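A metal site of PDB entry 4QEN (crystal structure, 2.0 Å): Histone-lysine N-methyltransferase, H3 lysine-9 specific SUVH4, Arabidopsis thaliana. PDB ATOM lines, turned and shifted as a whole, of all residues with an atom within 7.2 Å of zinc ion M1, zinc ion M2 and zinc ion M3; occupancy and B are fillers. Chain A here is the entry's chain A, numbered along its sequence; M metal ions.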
ATOM      1  N   THR A 290      33.735  32.540  -3.690  1.00  0.00           N
ATOM      2  CA  THR A 290      34.653  31.736  -4.473  1.00  0.00           C
ATOM      3  C   THR A 290      34.122  31.449  -5.885  1.00  0.00           C
ATOM      4  O   THR A 290      34.854  31.541  -6.870  1.00  0.00           O
ATOM      5  CB  THR A 290      34.978  30.416  -3.753  1.00  0.00           C
ATOM      6  OG1 THR A 290      35.571  30.704  -2.483  1.00  0.00           O
ATOM      7  CG2 THR A 290      35.921  29.571  -4.577  1.00  0.00           C
ATOM      8  N   GLY A 291      32.843  31.090  -5.988  1.00  0.00           N
ATOM      9  CA  GLY A 291      32.251  30.833  -7.291  1.00  0.00           C
ATOM     10  C   GLY A 291      32.527  29.447  -7.875  1.00  0.00           C
ATOM     11  O   GLY A 291      33.177  28.605  -7.264  1.00  0.00           O
ATOM     12  N   CYS A 292      32.027  29.229  -9.094  1.00  0.00           N
ATOM     13  CA  CYS A 292      32.096  27.913  -9.723  1.00  0.00           C
ATOM     14  C   CYS A 292      33.082  27.961 -10.884  1.00  0.00           C
ATOM     15  O   CYS A 292      33.509  29.049 -11.292  1.00  0.00           O
ATOM     16  CB  CYS A 292      30.705  27.514 -10.249  1.00  0.00           C
ATOM     17  SG  CYS A 292      30.066  28.594 -11.565  1.00  0.00           S
ATOM     18  N   ASN A 293      33.425  26.808 -11.430  1.00  0.00           N
ATOM     19  CA  ASN A 293      34.437  26.759 -12.483  1.00  0.00           C
ATOM     20  C   ASN A 293      33.848  26.412 -13.837  1.00  0.00           C
ATOM     21  O   ASN A 293      34.580  26.067 -14.770  1.00  0.00           O
ATOM     22  CB  ASN A 293      35.590  25.805 -12.115  1.00  0.00           C
ATOM     23  CG  ASN A 293      35.126  24.370 -11.908  1.00  0.00           C
ATOM     24  OD1 ASN A 293      34.040  23.978 -12.327  1.00  0.00           O
ATOM     25  ND2 ASN A 293      35.968  23.570 -11.251  1.00  0.00           N
ATOM     26  N   CYS A 294      32.520  26.476 -13.923  1.00  0.00           N
ATOM     27  CA  CYS A 294      31.829  26.177 -15.159  1.00  0.00           C
ATOM     28  C   CYS A 294      32.255  27.172 -16.225  1.00  0.00           C
ATOM     29  O   CYS A 294      32.728  28.261 -15.910  1.00  0.00           O
ATOM     30  CB  CYS A 294      30.306  26.245 -14.965  1.00  0.00           C
ATOM     31  SG  CYS A 294      29.688  25.230 -13.592  1.00  0.00           S
ATOM     32  N   ARG A 295      32.087  26.801 -17.483  1.00  0.00           N
ATOM     33  CA  ARG A 295      32.503  27.663 -18.568  1.00  0.00           C
ATOM     34  C   ARG A 295      31.330  28.075 -19.446  1.00  0.00           C
ATOM     35  O   ARG A 295      30.574  27.236 -19.921  1.00  0.00           O
ATOM     36  CB  ARG A 295      33.579  26.979 -19.405  1.00  0.00           C
ATOM     37  CG  ARG A 295      34.463  27.934 -20.151  1.00  0.00           C
ATOM     38  CD  ARG A 295      35.780  27.296 -20.506  1.00  0.00           C
ATOM     39  NE  ARG A 295      36.356  27.897 -21.695  1.00  0.00           N
ATOM     40  CZ  ARG A 295      36.994  29.059 -21.712  1.00  0.00           C
ATOM     41  NH1 ARG A 295      37.483  29.534 -22.844  1.00  0.00           N
ATOM     42  NH2 ARG A 295      37.146  29.741 -20.585  1.00  0.00           N
ATOM     43  N   GLY A 296      31.180  29.380 -19.649  1.00  0.00           N
ATOM     44  CA  GLY A 296      30.126  29.888 -20.511  1.00  0.00           C
ATOM     45  C   GLY A 296      28.809  30.053 -19.795  1.00  0.00           C
ATOM     46  O   GLY A 296      28.446  31.172 -19.435  1.00  0.00           O
ATOM     47  N   SER A 297      28.088  28.956 -19.616  1.00  0.00           N
ATOM     48  CA  SER A 297      26.818  28.960 -18.881  1.00  0.00           C
ATOM     49  C   SER A 297      26.773  27.772 -17.948  1.00  0.00           C
ATOM     50  O   SER A 297      27.244  26.691 -18.299  1.00  0.00           O
ATOM     51  CB  SER A 297      25.634  28.887 -19.839  1.00  0.00           C
ATOM     52  OG  SER A 297      25.386  30.134 -20.469  1.00  0.00           O
ATOM     53  N   CYS A 298      26.189  27.937 -16.775  1.00  0.00           N
ATOM     54  CA  CYS A 298      26.094  26.809 -15.850  1.00  0.00           C
ATOM     55  C   CYS A 298      24.852  25.954 -16.120  1.00  0.00           C
ATOM     56  O   CYS A 298      23.731  26.448 -16.048  1.00  0.00           O
ATOM     57  CB  CYS A 298      26.119  27.297 -14.408  1.00  0.00           C
ATOM     58  SG  CYS A 298      27.601  28.226 -14.104  1.00  0.00           S
ATOM     59  N   THR A 299      25.080  24.683 -16.463  1.00  0.00           N
ATOM     60  CA  THR A 299      23.971  23.787 -16.825  1.00  0.00           C
ATOM     61  C   THR A 299      24.023  22.432 -16.120  1.00  0.00           C
ATOM     62  O   THR A 299      23.003  21.753 -15.986  1.00  0.00           O
ATOM     63  CB  THR A 299      23.898  23.536 -18.344  1.00  0.00           C
ATOM     64  OG1 THR A 299      25.210  23.221 -18.826  1.00  0.00           O
ATOM     65  CG2 THR A 299      23.382  24.778 -19.064  1.00  0.00           C
ATOM     66  N   ASP A 300      25.208  22.032 -15.677  1.00  0.00           N
ATOM     67  CA  ASP A 300      25.362  20.774 -14.967  1.00  0.00           C
ATOM     68  C   ASP A 300      25.386  21.032 -13.465  1.00  0.00           C
ATOM     69  O   ASP A 300      26.360  21.547 -12.921  1.00  0.00           O
ATOM     70  CB  ASP A 300      26.635  20.062 -15.425  1.00  0.00           C
ATOM     71  CG  ASP A 300      26.751  18.654 -14.871  1.00  0.00           C
ATOM     72  OD1 ASP A 300      26.513  18.456 -13.663  1.00  0.00           O
ATOM     73  OD2 ASP A 300      27.074  17.728 -15.658  1.00  0.00           O
ATOM     74  N   LYS A 303      28.400  19.525 -11.346  1.00  0.00           N
ATOM     75  CA  LYS A 303      29.730  20.114 -11.428  1.00  0.00           C
ATOM     76  C   LYS A 303      29.783  21.539 -10.873  1.00  0.00           C
ATOM     77  O   LYS A 303      30.866  22.042 -10.577  1.00  0.00           O
ATOM     78  CB  LYS A 303      30.230  20.109 -12.881  1.00  0.00           C
ATOM     79  CG  LYS A 303      30.210  18.739 -13.546  1.00  0.00           C
ATOM     80  CD  LYS A 303      31.140  18.717 -14.758  1.00  0.00           C
ATOM     81  CE  LYS A 303      30.547  17.914 -15.917  1.00  0.00           C
ATOM     82  NZ  LYS A 303      29.376  18.633 -16.533  1.00  0.00           N
ATOM     83  N   CYS A 304      28.627  22.172 -10.751  1.00  0.00           N
ATOM     84  CA  CYS A 304      28.530  23.594 -10.401  1.00  0.00           C
ATOM     85  C   CYS A 304      28.402  23.859  -8.907  1.00  0.00           C
ATOM     86  O   CYS A 304      27.387  23.536  -8.298  1.00  0.00           O
ATOM     87  CB  CYS A 304      27.342  24.225 -11.126  1.00  0.00           C
ATOM     88  SG  CYS A 304      27.094  25.997 -10.745  1.00  0.00           S
ATOM     89  N   ALA A 305      29.428  24.473  -8.322  1.00  0.00           N
ATOM     90  CA  ALA A 305      29.417  24.820  -6.897  1.00  0.00           C
ATOM     91  C   ALA A 305      28.248  25.740  -6.511  1.00  0.00           C
ATOM     92  O   ALA A 305      27.765  25.727  -5.365  1.00  0.00           O
ATOM     93  CB  ALA A 305      30.753  25.463  -6.508  1.00  0.00           C
ATOM     94  N   CYS A 306      27.788  26.529  -7.470  1.00  0.00           N
ATOM     95  CA  CYS A 306      26.717  27.480  -7.220  1.00  0.00           C
ATOM     96  C   CYS A 306      25.355  26.775  -7.177  1.00  0.00           C
ATOM     97  O   CYS A 306      24.475  27.167  -6.411  1.00  0.00           O
ATOM     98  CB  CYS A 306      26.750  28.612  -8.249  1.00  0.00           C
ATOM     99  SG  CYS A 306      28.312  29.584  -8.247  1.00  0.00           S
ATOM    100  N   ALA A 307      25.195  25.727  -7.971  1.00  0.00           N
ATOM    101  CA  ALA A 307      24.015  24.872  -7.857  1.00  0.00           C
ATOM    102  C   ALA A 307      24.052  24.152  -6.510  1.00  0.00           C
ATOM    103  O   ALA A 307      23.015  23.970  -5.870  1.00  0.00           O
ATOM    104  CB  ALA A 307      23.963  23.859  -9.010  1.00  0.00           C
ATOM    105  N   PHE A 314      19.412  24.167  -9.774  1.00  0.00           N
ATOM    106  CA  PHE A 314      19.357  25.589 -10.080  1.00  0.00           C
ATOM    107  C   PHE A 314      18.006  26.144  -9.653  1.00  0.00           C
ATOM    108  O   PHE A 314      16.983  25.488  -9.828  1.00  0.00           O
ATOM    109  CB  PHE A 314      19.621  25.816 -11.569  1.00  0.00           C
ATOM    110  CG  PHE A 314      21.039  25.493 -11.976  1.00  0.00           C
ATOM    111  CD1 PHE A 314      22.067  26.382 -11.711  1.00  0.00           C
ATOM    112  CD2 PHE A 314      21.337  24.299 -12.603  1.00  0.00           C
ATOM    113  CE1 PHE A 314      23.385  26.078 -12.077  1.00  0.00           C
ATOM    114  CE2 PHE A 314      22.638  23.996 -12.980  1.00  0.00           C
ATOM    115  CZ  PHE A 314      23.659  24.889 -12.703  1.00  0.00           C
ATOM    116  N   PHE A 332      21.298  31.614  -4.378  1.00  0.00           N
ATOM    117  CA  PHE A 332      22.724  31.826  -4.625  1.00  0.00           C
ATOM    118  C   PHE A 332      23.013  31.909  -6.115  1.00  0.00           C
ATOM    119  O   PHE A 332      22.944  30.900  -6.824  1.00  0.00           O
ATOM    120  CB  PHE A 332      23.551  30.703  -4.004  1.00  0.00           C
ATOM    121  CG  PHE A 332      23.476  30.652  -2.502  1.00  0.00           C
ATOM    122  CD1 PHE A 332      24.388  31.342  -1.727  1.00  0.00           C
ATOM    123  CD2 PHE A 332      22.494  29.894  -1.872  1.00  0.00           C
ATOM    124  CE1 PHE A 332      24.321  31.285  -0.341  1.00  0.00           C
ATOM    125  CE2 PHE A 332      22.421  29.829  -0.496  1.00  0.00           C
ATOM    126  CZ  PHE A 332      23.338  30.524   0.272  1.00  0.00           C
ATOM    127  N   GLU A 333      23.317  33.106  -6.595  1.00  0.00           N
ATOM    128  CA  GLU A 333      23.626  33.329  -8.009  1.00  0.00           C
ATOM    129  C   GLU A 333      25.123  33.254  -8.271  1.00  0.00           C
ATOM    130  O   GLU A 333      25.919  33.450  -7.356  1.00  0.00           O
ATOM    131  CB  GLU A 333      23.101  34.688  -8.472  1.00  0.00           C
ATOM    132  CG  GLU A 333      21.609  34.679  -8.840  1.00  0.00           C
ATOM    133  CD  GLU A 333      21.112  36.039  -9.310  1.00  0.00           C
ATOM    134  OE1 GLU A 333      21.900  37.013  -9.355  1.00  0.00           O
ATOM    135  OE2 GLU A 333      19.914  36.124  -9.632  1.00  0.00           O
ATOM    136  N   CYS A 334      25.496  32.987  -9.521  1.00  0.00           N
ATOM    137  CA  CYS A 334      26.897  33.074  -9.940  1.00  0.00           C
ATOM    138  C   CYS A 334      27.360  34.532  -9.795  1.00  0.00           C
ATOM    139  O   CYS A 334      26.525  35.452  -9.798  1.00  0.00           O
ATOM    140  CB  CYS A 334      27.066  32.563 -11.367  1.00  0.00           C
ATOM    141  SG  CYS A 334      26.735  30.793 -11.514  1.00  0.00           S
ATOM    142  N   GLY A 335      28.666  34.732  -9.644  1.00  0.00           N
ATOM    143  CA  GLY A 335      29.198  36.051  -9.332  1.00  0.00           C
ATOM    144  C   GLY A 335      30.521  36.351 -10.017  1.00  0.00           C
ATOM    145  O   GLY A 335      30.884  35.686 -10.987  1.00  0.00           O
ATOM    146  N   HIS A 337      33.590  35.838  -9.643  1.00  0.00           N
ATOM    147  CA  HIS A 337      34.668  34.861  -9.819  1.00  0.00           C
ATOM    148  C   HIS A 337      34.228  33.580 -10.503  1.00  0.00           C
ATOM    149  O   HIS A 337      35.031  32.666 -10.680  1.00  0.00           O
ATOM    150  CB  HIS A 337      35.345  34.551  -8.481  1.00  0.00           C
ATOM    151  CG  HIS A 337      36.101  35.706  -7.915  1.00  0.00           C
ATOM    152  ND1 HIS A 337      37.164  36.284  -8.561  1.00  0.00           N
ATOM    153  CD2 HIS A 337      35.939  36.397  -6.757  1.00  0.00           C
ATOM    154  CE1 HIS A 337      37.639  37.286  -7.840  1.00  0.00           C
ATOM    155  NE2 HIS A 337      36.910  37.375  -6.732  1.00  0.00           N
ATOM    156  N   CYS A 338      32.960  33.502 -10.884  1.00  0.00           N
ATOM    157  CA  CYS A 338      32.512  32.305 -11.598  1.00  0.00           C
ATOM    158  C   CYS A 338      33.102  32.290 -13.006  1.00  0.00           C
ATOM    159  O   CYS A 338      33.372  33.339 -13.579  1.00  0.00           O
ATOM    160  CB  CYS A 338      30.991  32.240 -11.635  1.00  0.00           C
ATOM    161  SG  CYS A 338      30.288  32.025  -9.989  1.00  0.00           S
ATOM    162  N   GLY A 339      33.298  31.108 -13.555  1.00  0.00           N
ATOM    163  CA  GLY A 339      33.838  30.988 -14.904  1.00  0.00           C
ATOM    164  C   GLY A 339      32.812  31.263 -15.992  1.00  0.00           C
ATOM    165  O   GLY A 339      33.169  31.354 -17.176  1.00  0.00           O
ATOM    166  N   CYS A 340      31.549  31.404 -15.619  1.00  0.00           N
ATOM    167  CA  CYS A 340      30.485  31.596 -16.594  1.00  0.00           C
ATOM    168  C   CYS A 340      30.306  33.064 -16.945  1.00  0.00           C
ATOM    169  O   CYS A 340      30.656  33.941 -16.165  1.00  0.00           O
ATOM    170  CB  CYS A 340      29.158  31.071 -16.037  1.00  0.00           C
ATOM    171  SG  CYS A 340      28.688  31.928 -14.521  1.00  0.00           S
ATOM    172  N   GLY A 341      29.745  33.311 -18.125  1.00  0.00           N
ATOM    173  CA  GLY A 341      29.484  34.659 -18.600  1.00  0.00           C
ATOM    174  C   GLY A 341      28.068  35.116 -18.267  1.00  0.00           C
ATOM    175  O   GLY A 341      27.297  34.374 -17.640  1.00  0.00           O
ATOM    176  N   LYS A 343      25.299  35.376 -19.715  1.00  0.00           N
ATOM    177  CA  LYS A 343      24.111  34.665 -20.203  1.00  0.00           C
ATOM    178  C   LYS A 343      23.669  33.549 -19.269  1.00  0.00           C
ATOM    179  O   LYS A 343      22.555  33.043 -19.400  1.00  0.00           O
ATOM    180  CB  LYS A 343      24.356  34.092 -21.605  1.00  0.00           C
ATOM    181  CG  LYS A 343      24.340  35.124 -22.716  1.00  0.00           C
ATOM    182  CD  LYS A 343      24.368  34.447 -24.083  1.00  0.00           C
ATOM    183  CE  LYS A 343      24.414  35.472 -25.212  1.00  0.00           C
ATOM    184  NZ  LYS A 343      24.563  34.820 -26.541  1.00  0.00           N
ATOM    185  N   CYS A 344      24.529  33.174 -18.323  1.00  0.00           N
ATOM    186  CA  CYS A 344      24.214  32.109 -17.372  1.00  0.00           C
ATOM    187  C   CYS A 344      22.841  32.267 -16.718  1.00  0.00           C
ATOM    188  O   CYS A 344      22.476  33.353 -16.253  1.00  0.00           O
ATOM    189  CB  CYS A 344      25.277  32.017 -16.279  1.00  0.00           C
ATOM    190  SG  CYS A 344      24.935  30.698 -15.129  1.00  0.00           S
ATOM    191  N   VAL A 345      22.079  31.191 -16.687  1.00  0.00           N
ATOM    192  CA  VAL A 345      20.716  31.270 -16.143  1.00  0.00           C
ATOM    193  C   VAL A 345      20.765  31.504 -14.626  1.00  0.00           C
ATOM    194  O   VAL A 345      19.877  32.144 -14.046  1.00  0.00           O
ATOM    195  CB  VAL A 345      19.890  30.019 -16.498  1.00  0.00           C
ATOM    196  CG1 VAL A 345      18.474  30.105 -15.930  1.00  0.00           C
ATOM    197  CG2 VAL A 345      19.823  29.881 -18.030  1.00  0.00           C
ATOM    198  N   ASN A 346      21.840  31.055 -13.997  1.00  0.00           N
ATOM    199  CA  ASN A 346      22.039  31.329 -12.584  1.00  0.00           C
ATOM    200  C   ASN A 346      22.575  32.752 -12.336  1.00  0.00           C
ATOM    201  O   ASN A 346      23.098  33.043 -11.264  1.00  0.00           O
ATOM    202  CB  ASN A 346      22.931  30.261 -11.945  1.00  0.00           C
ATOM    203  CG  ASN A 346      22.665  30.107 -10.461  1.00  0.00           C
ATOM    204  OD1 ASN A 346      21.525  30.136 -10.034  1.00  0.00           O
ATOM    205  ND2 ASN A 346      23.734  29.964  -9.665  1.00  0.00           N
ATOM    206  N   ARG A 347      22.457  33.629 -13.320  1.00  0.00           N
ATOM    207  CA  ARG A 347      22.623  35.057 -13.102  1.00  0.00           C
ATOM    208  C   ARG A 347      21.347  35.790 -13.495  1.00  0.00           C
ATOM    209  O   ARG A 347      21.383  36.959 -13.893  1.00  0.00           O
ATOM    210  CB  ARG A 347      23.776  35.630 -13.930  1.00  0.00           C
ATOM    211  CG  ARG A 347      25.146  35.048 -13.616  1.00  0.00           C
ATOM    212  CD  ARG A 347      26.163  35.586 -14.604  1.00  0.00           C
ATOM    213  NE  ARG A 347      27.502  35.040 -14.418  1.00  0.00           N
ATOM    214  CZ  ARG A 347      28.398  35.587 -13.603  1.00  0.00           C
ATOM    215  NH1 ARG A 347      28.069  36.666 -12.910  1.00  0.00           N
ATOM    216  NH2 ARG A 347      29.620  35.059 -13.492  1.00  0.00           N
HETATM  217 ZN    ZN M   1      26.957  30.555 -13.840  1.00  0.00          ZN
HETATM  218 ZN    ZN M   2      28.772  30.140 -10.379  1.00  0.00          ZN
HETATM  219 ZN    ZN M   3      28.511  26.963 -12.410  1.00  0.00          ZN
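Zinc ion M2 is bound by the side-chain sulfur (SG) of Cys 306 (2.3 Å). Zinc ion M2 is bound by SG of Cys 292 (2.3 Å). Zinc ion M2 is bound by the side-chain sulfur (SG) of Cys 334 (2.4 Å). Zinc ion M2 is bound by SG of Cys 338, at 2.5 Å.
The backbone NH (N) of Gly 339 lies within hydrogen-bond range of the backbone carbonyl oxygen (O) of Cys 292, at 3.1 Å. The backbone carbonyl oxygen (O) of Cys 294 sits at hydrogen-bond distance from the backbone NH (N) of Cys 340 (3.4 Å). N of Gly 335 lies close to SG of Cys 338, at 3.2 Å. The backbone NH (N) of Cys 334 sits at hydrogen-bond distance from the backbone carbonyl oxygen (O) of Asn 346 (3.0 Å). The backbone carbonyl oxygen of Cys 340 sits at hydrogen-bond distance from the guanidinium group of Arg 347 (3.1 Å). The backbone NH of Cys 306 lies close to the side-chain sulfur of Cys 304 (3.4 Å). SG of Cys 304 lies close to N of Ala 307 (3.4 Å). The backbone NH (N) of Asn 346 lies close to the side-chain sulfur (SG) of Cys 344 (3.3 Å).
Within 4 Å of zinc ion M2: Cys 292, Cys 306, Cys 334 and Cys 338. The nearest printed residue that does not touch zinc ion M2 is Cys 298 (4.3 Å).
Zinc ion M1 is bound by SG of Cys 340 (2.3 Å), SG of Cys 334 (2.3 Å), SG of Cys 344 (2.4 Å) and SG of Cys 298 (2.4 Å).
The nearest printed residue that does not touch zinc ion M1 is Cys 292 (4.3 Å).
Zinc ion M3 is bound by SG of Cys 298, SG of Cys 304, SG of Cys 294 and SG of Cys 292.
Of the 31 residues printed, 4 come within 4 Å of zinc ion M3.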
